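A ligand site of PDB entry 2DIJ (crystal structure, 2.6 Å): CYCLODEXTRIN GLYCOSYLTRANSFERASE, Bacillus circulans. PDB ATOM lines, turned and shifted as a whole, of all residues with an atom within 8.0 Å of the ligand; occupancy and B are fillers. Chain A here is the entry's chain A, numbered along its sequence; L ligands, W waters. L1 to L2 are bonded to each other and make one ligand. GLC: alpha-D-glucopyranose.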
ATOM      1  N   TYR A 301     -12.609 -21.234   7.031  1.00  0.00           N
ATOM      2  CA  TYR A 301     -12.411 -21.399   5.606  1.00  0.00           C
ATOM      3  C   TYR A 301     -13.128 -20.312   4.841  1.00  0.00           C
ATOM      4  O   TYR A 301     -12.612 -19.776   3.851  1.00  0.00           O
ATOM      5  CB  TYR A 301     -12.748 -22.814   5.121  1.00  0.00           C
ATOM      6  CG  TYR A 301     -11.832 -23.827   5.763  1.00  0.00           C
ATOM      7  CD1 TYR A 301     -10.530 -24.010   5.299  1.00  0.00           C
ATOM      8  CD2 TYR A 301     -12.259 -24.562   6.873  1.00  0.00           C
ATOM      9  CE1 TYR A 301      -9.673 -24.929   5.905  1.00  0.00           C
ATOM     10  CE2 TYR A 301     -11.409 -25.483   7.491  1.00  0.00           C
ATOM     11  CZ  TYR A 301     -10.117 -25.664   6.999  1.00  0.00           C
ATOM     12  OH  TYR A 301      -9.288 -26.556   7.606  1.00  0.00           O
ATOM     13  N   LYS A 304     -11.198 -17.107   5.250  1.00  0.00           N
ATOM     14  CA  LYS A 304     -10.056 -17.112   4.352  1.00  0.00           C
ATOM     15  C   LYS A 304     -10.453 -16.832   2.914  1.00  0.00           C
ATOM     16  O   LYS A 304      -9.779 -16.091   2.202  1.00  0.00           O
ATOM     17  CB  LYS A 304      -9.216 -18.369   4.481  1.00  0.00           C
ATOM     18  CG  LYS A 304      -8.388 -18.639   3.236  1.00  0.00           C
ATOM     19  CD  LYS A 304      -7.630 -19.962   3.330  1.00  0.00           C
ATOM     20  CE  LYS A 304      -6.956 -20.362   2.024  1.00  0.00           C
ATOM     21  NZ  LYS A 304      -5.487 -20.474   2.151  1.00  0.00           N
ATOM     22  N   GLN A 410      -1.858 -13.160   4.165  1.00  0.00           N
ATOM     23  CA  GLN A 410      -1.556 -14.529   3.804  1.00  0.00           C
ATOM     24  C   GLN A 410      -1.860 -15.506   4.912  1.00  0.00           C
ATOM     25  O   GLN A 410      -1.386 -15.374   6.037  1.00  0.00           O
ATOM     26  CB  GLN A 410      -0.085 -14.652   3.375  1.00  0.00           C
ATOM     27  CG  GLN A 410       0.286 -16.055   2.870  1.00  0.00           C
ATOM     28  CD  GLN A 410       1.780 -16.255   2.782  1.00  0.00           C
ATOM     29  OE1 GLN A 410       2.262 -17.227   2.176  1.00  0.00           O
ATOM     30  NE2 GLN A 410       2.537 -15.347   3.400  1.00  0.00           N
ATOM     31  N   GLU A 411      -2.637 -16.522   4.586  1.00  0.00           N
ATOM     32  CA  GLU A 411      -2.977 -17.541   5.557  1.00  0.00           C
ATOM     33  C   GLU A 411      -1.769 -18.443   5.809  1.00  0.00           C
ATOM     34  O   GLU A 411      -1.167 -18.964   4.863  1.00  0.00           O
ATOM     35  CB  GLU A 411      -4.187 -18.366   5.112  1.00  0.00           C
ATOM     36  CG  GLU A 411      -4.411 -19.627   5.959  1.00  0.00           C
ATOM     37  CD  GLU A 411      -3.746 -20.833   5.372  1.00  0.00           C
ATOM     38  OE1 GLU A 411      -3.912 -21.207   4.226  1.00  0.00           O
ATOM     39  OE2 GLU A 411      -2.954 -21.435   6.221  1.00  0.00           O
ATOM     40  N   ARG A 412      -1.399 -18.615   7.077  1.00  0.00           N
ATOM     41  CA  ARG A 412      -0.252 -19.457   7.411  1.00  0.00           C
ATOM     42  C   ARG A 412      -0.600 -20.732   8.168  1.00  0.00           C
ATOM     43  O   ARG A 412       0.178 -21.690   8.205  1.00  0.00           O
ATOM     44  CB  ARG A 412       0.884 -18.667   8.053  1.00  0.00           C
ATOM     45  CG  ARG A 412       1.011 -17.275   7.462  1.00  0.00           C
ATOM     46  CD  ARG A 412       2.425 -16.923   7.023  1.00  0.00           C
ATOM     47  NE  ARG A 412       3.042 -17.933   6.183  1.00  0.00           N
ATOM     48  CZ  ARG A 412       4.189 -17.742   5.523  1.00  0.00           C
ATOM     49  NH1 ARG A 412       4.862 -16.599   5.579  1.00  0.00           N
ATOM     50  NH2 ARG A 412       4.681 -18.737   4.789  1.00  0.00           N
ATOM     51  N   TRP A 413      -1.794 -20.758   8.751  1.00  0.00           N
ATOM     52  CA  TRP A 413      -2.311 -21.898   9.495  1.00  0.00           C
ATOM     53  C   TRP A 413      -3.818 -21.779   9.558  1.00  0.00           C
ATOM     54  O   TRP A 413      -4.359 -20.693   9.769  1.00  0.00           O
ATOM     55  CB  TRP A 413      -1.709 -21.979  10.912  1.00  0.00           C
ATOM     56  CG  TRP A 413      -1.535 -23.375  11.463  1.00  0.00           C
ATOM     57  CD1 TRP A 413      -0.379 -24.088  11.467  1.00  0.00           C
ATOM     58  CD2 TRP A 413      -2.496 -24.186  12.156  1.00  0.00           C
ATOM     59  NE1 TRP A 413      -0.564 -25.298  12.075  1.00  0.00           N
ATOM     60  CE2 TRP A 413      -1.848 -25.384  12.507  1.00  0.00           C
ATOM     61  CE3 TRP A 413      -3.839 -24.016  12.488  1.00  0.00           C
ATOM     62  CZ2 TRP A 413      -2.508 -26.402  13.192  1.00  0.00           C
ATOM     63  CZ3 TRP A 413      -4.493 -25.032  13.160  1.00  0.00           C
ATOM     64  CH2 TRP A 413      -3.829 -26.216  13.506  1.00  0.00           C
ATOM     65  N   ILE A 414      -4.514 -22.903   9.377  1.00  0.00           N
ATOM     66  CA  ILE A 414      -5.952 -22.821   9.407  1.00  0.00           C
ATOM     67  C   ILE A 414      -6.652 -24.144   9.614  1.00  0.00           C
ATOM     68  O   ILE A 414      -6.215 -25.186   9.161  1.00  0.00           O
ATOM     69  CB  ILE A 414      -6.468 -22.183   8.128  1.00  0.00           C
ATOM     70  CG1 ILE A 414      -7.979 -22.091   8.183  1.00  0.00           C
ATOM     71  CG2 ILE A 414      -6.038 -23.031   6.940  1.00  0.00           C
ATOM     72  CD1 ILE A 414      -8.603 -21.795   6.830  1.00  0.00           C
ATOM     73  N   ASN A 415      -7.796 -24.049  10.264  1.00  0.00           N
ATOM     74  CA  ASN A 415      -8.690 -25.156  10.520  1.00  0.00           C
ATOM     75  C   ASN A 415     -10.096 -24.623  10.695  1.00  0.00           C
ATOM     76  O   ASN A 415     -10.365 -23.468  10.394  1.00  0.00           O
ATOM     77  CB  ASN A 415      -8.222 -26.126  11.637  1.00  0.00           C
ATOM     78  CG  ASN A 415      -8.559 -25.733  13.069  1.00  0.00           C
ATOM     79  OD1 ASN A 415      -9.264 -24.759  13.337  1.00  0.00           O
ATOM     80  ND2 ASN A 415      -8.049 -26.526  14.000  1.00  0.00           N
ATOM     81  N   ASN A 416     -10.984 -25.433  11.199  1.00  0.00           N
ATOM     82  CA  ASN A 416     -12.347 -24.977  11.383  1.00  0.00           C
ATOM     83  C   ASN A 416     -12.465 -23.713  12.223  1.00  0.00           C
ATOM     84  O   ASN A 416     -13.174 -22.781  11.845  1.00  0.00           O
ATOM     85  CB  ASN A 416     -13.232 -26.079  11.963  1.00  0.00           C
ATOM     86  CG  ASN A 416     -13.647 -27.111  10.946  1.00  0.00           C
ATOM     87  OD1 ASN A 416     -14.313 -28.094  11.272  1.00  0.00           O
ATOM     88  ND2 ASN A 416     -13.247 -26.889   9.695  1.00  0.00           N
ATOM     89  N   VAL A 418      -9.555 -22.126  13.834  1.00  0.00           N
ATOM     90  CA  VAL A 418      -8.326 -21.370  13.954  1.00  0.00           C
ATOM     91  C   VAL A 418      -7.905 -20.695  12.677  1.00  0.00           C
ATOM     92  O   VAL A 418      -8.116 -21.205  11.582  1.00  0.00           O
ATOM     93  CB  VAL A 418      -7.193 -22.263  14.461  1.00  0.00           C
ATOM     94  CG1 VAL A 418      -5.924 -21.443  14.693  1.00  0.00           C
ATOM     95  CG2 VAL A 418      -7.612 -22.956  15.750  1.00  0.00           C
ATOM     96  N   ILE A 420      -4.446 -18.335  11.490  1.00  0.00           N
ATOM     97  CA  ILE A 420      -3.225 -17.618  11.716  1.00  0.00           C
ATOM     98  C   ILE A 420      -2.826 -16.984  10.411  1.00  0.00           C
ATOM     99  O   ILE A 420      -2.532 -17.685   9.451  1.00  0.00           O
ATOM    100  CB  ILE A 420      -2.122 -18.502  12.282  1.00  0.00           C
ATOM    101  CG1 ILE A 420      -2.641 -19.225  13.520  1.00  0.00           C
ATOM    102  CG2 ILE A 420      -0.916 -17.645  12.646  1.00  0.00           C
ATOM    103  CD1 ILE A 420      -1.548 -20.016  14.230  1.00  0.00           C
ATOM    104  N   SER A 443      -3.756 -27.239  19.008  1.00  0.00           N
ATOM    105  CA  SER A 443      -2.343 -27.560  18.989  1.00  0.00           C
ATOM    106  C   SER A 443      -1.762 -27.072  17.684  1.00  0.00           C
ATOM    107  O   SER A 443      -2.083 -27.593  16.608  1.00  0.00           O
ATOM    108  CB  SER A 443      -2.077 -29.035  19.191  1.00  0.00           C
ATOM    109  OG  SER A 443      -1.053 -29.202  20.143  1.00  0.00           O
ATOM    110  N   ILE A 444      -0.917 -26.069  17.769  1.00  0.00           N
ATOM    111  CA  ILE A 444      -0.333 -25.521  16.583  1.00  0.00           C
ATOM    112  C   ILE A 444       1.093 -25.954  16.338  1.00  0.00           C
ATOM    113  O   ILE A 444       1.999 -25.687  17.125  1.00  0.00           O
ATOM    114  CB  ILE A 444      -0.496 -24.022  16.473  1.00  0.00           C
ATOM    115  CG1 ILE A 444      -1.972 -23.701  16.226  1.00  0.00           C
ATOM    116  CG2 ILE A 444       0.348 -23.480  15.324  1.00  0.00           C
ATOM    117  CD1 ILE A 444      -2.664 -23.148  17.456  1.00  0.00           C
ATOM    118  N   SER A 445       1.263 -26.641  15.221  1.00  0.00           N
ATOM    119  CA  SER A 445       2.548 -27.116  14.768  1.00  0.00           C
ATOM    120  C   SER A 445       2.611 -26.990  13.264  1.00  0.00           C
ATOM    121  O   SER A 445       1.588 -27.117  12.591  1.00  0.00           O
ATOM    122  CB  SER A 445       2.886 -28.525  15.231  1.00  0.00           C
ATOM    123  OG  SER A 445       1.745 -29.350  15.150  1.00  0.00           O
ATOM    124  N   GLY A 446       3.784 -26.698  12.750  1.00  0.00           N
ATOM    125  CA  GLY A 446       3.958 -26.551  11.316  1.00  0.00           C
ATOM    126  C   GLY A 446       3.785 -25.108  10.880  1.00  0.00           C
ATOM    127  O   GLY A 446       3.753 -24.796   9.694  1.00  0.00           O
ATOM    128  N   LEU A 447       3.675 -24.225  11.863  1.00  0.00           N
ATOM    129  CA  LEU A 447       3.518 -22.818  11.561  1.00  0.00           C
ATOM    130  C   LEU A 447       4.794 -22.225  10.989  1.00  0.00           C
ATOM    131  O   LEU A 447       5.851 -22.253  11.610  1.00  0.00           O
ATOM    132  CB  LEU A 447       3.057 -22.017  12.795  1.00  0.00           C
ATOM    133  CG  LEU A 447       3.140 -20.513  12.568  1.00  0.00           C
ATOM    134  CD1 LEU A 447       2.218 -20.110  11.430  1.00  0.00           C
ATOM    135  CD2 LEU A 447       2.743 -19.780  13.846  1.00  0.00           C
ATOM    136  N   VAL A 448       4.664 -21.659   9.803  1.00  0.00           N
ATOM    137  CA  VAL A 448       5.784 -21.025   9.148  1.00  0.00           C
ATOM    138  C   VAL A 448       5.469 -19.565   8.921  1.00  0.00           C
ATOM    139  O   VAL A 448       4.383 -19.227   8.449  1.00  0.00           O
ATOM    140  CB  VAL A 448       6.154 -21.700   7.839  1.00  0.00           C
ATOM    141  CG1 VAL A 448       7.410 -21.046   7.274  1.00  0.00           C
ATOM    142  CG2 VAL A 448       6.403 -23.184   8.078  1.00  0.00           C
ATOM    143  N   THR A 449       6.411 -18.692   9.265  1.00  0.00           N
ATOM    144  CA  THR A 449       6.192 -17.266   9.106  1.00  0.00           C
ATOM    145  C   THR A 449       7.350 -16.559   8.461  1.00  0.00           C
ATOM    146  O   THR A 449       8.382 -17.158   8.150  1.00  0.00           O
ATOM    147  CB  THR A 449       5.915 -16.617  10.474  1.00  0.00           C
ATOM    148  OG1 THR A 449       7.146 -16.468  11.166  1.00  0.00           O
ATOM    149  CG2 THR A 449       4.980 -17.508  11.271  1.00  0.00           C
ATOM    150  N   ALA A 476      10.420 -20.838  11.040  1.00  0.00           N
ATOM    151  CA  ALA A 476       9.623 -21.918  11.578  1.00  0.00           C
ATOM    152  C   ALA A 476       9.343 -21.735  13.057  1.00  0.00           C
ATOM    153  O   ALA A 476      10.263 -21.653  13.879  1.00  0.00           O
ATOM    154  CB  ALA A 476      10.277 -23.262  11.326  1.00  0.00           C
HETATM  155  C1  GLC L   1      -2.501 -28.303  10.051  1.00  0.00           C
HETATM  156  C2  GLC L   1      -3.230 -27.051   9.661  1.00  0.00           C
HETATM  157  C3  GLC L   1      -2.670 -26.479   8.382  1.00  0.00           C
HETATM  158  C4  GLC L   1      -1.165 -26.285   8.542  1.00  0.00           C
HETATM  159  C5  GLC L   1      -0.518 -27.617   8.916  1.00  0.00           C
HETATM  160  C6  GLC L   1       0.957 -27.483   9.168  1.00  0.00           C
HETATM  161  O1  GLC L   1      -2.807 -29.304   9.147  1.00  0.00           O
HETATM  162  O2  GLC L   1      -4.613 -27.330   9.473  1.00  0.00           O
HETATM  163  O3  GLC L   1      -3.342 -25.270   8.103  1.00  0.00           O
HETATM  164  O4  GLC L   1      -0.621 -25.866   7.284  1.00  0.00           O
HETATM  165  O5  GLC L   1      -1.097 -28.050  10.140  1.00  0.00           O
HETATM  166  O6  GLC L   1       1.487 -28.775   9.443  1.00  0.00           O
HETATM  167  C1  GLC L   2       0.040 -24.624   7.239  1.00  0.00           C
HETATM  168  C2  GLC L   2      -0.394 -23.887   5.987  1.00  0.00           C
HETATM  169  C3  GLC L   2       0.151 -24.562   4.766  1.00  0.00           C
HETATM  170  C4  GLC L   2       1.660 -24.699   4.857  1.00  0.00           C
HETATM  171  C5  GLC L   2       2.073 -25.383   6.143  1.00  0.00           C
HETATM  172  C6  GLC L   2       3.557 -25.257   6.365  1.00  0.00           C
HETATM  173  O2  GLC L   2      -1.808 -23.855   5.922  1.00  0.00           O
HETATM  174  O3  GLC L   2      -0.128 -23.779   3.603  1.00  0.00           O
HETATM  175  O4  GLC L   2       2.168 -25.497   3.788  1.00  0.00           O
HETATM  176  O5  GLC L   2       1.465 -24.771   7.283  1.00  0.00           O
HETATM  177  O6  GLC L   2       4.047 -26.131   7.379  1.00  0.00           O
HETATM  178  O   HOH W   1      -6.672 -26.907   7.115  1.00  0.00           O
HETATM  179  O   HOH W   2      -5.501 -29.588  10.714  1.00  0.00           O
HETATM  180  O   HOH W   3       2.772 -22.385   8.020  1.00  0.00           O
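The backbone carbonyl oxygen (O) of Gly 446 is in hydrogen-bond range of an oxygen (O6) of GLC L2. The side-chain carboxylate (OE2) of Glu 411 is in hydrogen-bond range of an oxygen (O2) of GLC L2. The backbone NH of Ile 414 sits at hydrogen-bond distance from an oxygen (O3) of GLC L1 (2.9 Å). O2 of GLC L1 is in hydrogen-bond range of O of Ile 414 (2.7 Å). The indole nitrogen (NE1) of Trp 413 is in hydrogen-bond range of an oxygen (O5) of GLC L1 (3.4 Å).
The side-chain carboxylate (OE2) of Glu 411 sits at hydrogen-bond distance from the backbone NH (N) of Trp 413. The side-chain amino group (NZ) of Lys 304 lies within salt-bridge range of the side-chain carboxylate (OE1) of Glu 411. The backbone carbonyl oxygen of Val 448 sits at hydrogen-bond distance from the guanidinium group of Arg 412, 2.9 Å away. The guanidinium group of Arg 412 sits close to the side-chain amide nitrogen of Gln 410. The backbone NH of Arg 412 lies within hydrogen-bond range of the backbone carbonyl oxygen of Ile 420, 2.8 Å away. O of Ser 445 sits at hydrogen-bond distance from NE1 of Trp 413 (2.9 Å). The backbone carbonyl oxygen (O) of Trp 413 sits at hydrogen-bond distance from the backbone NH (N) of Ile 420 (2.9 Å).
Water W1 lies within hydrogen-bond range of the side-chain hydroxyl of Tyr 301 (2.7 Å), the backbone carbonyl oxygen of Ile 414 (2.7 Å) and an oxygen (O2) of GLC L1 (3.2 Å).
An oxygen (O5) of GLC L2 lies close to the backbone carbonyl oxygen of Arg 412, at 3.5 Å. O of Ser 445 touches C6 of GLC L1, 3.5 Å away. CG2 of Val 448 touches O6 of GLC L2 (3.8 Å). Hydrophobic or aromatic side chains that line the ligand: Trp 413, Ile 414 and Val 448. Of the 19 residues printed, 7 come within 4 Å of the ligand. The nearest printed residue that does not touch the ligand is Asn 415 (4.4 Å).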
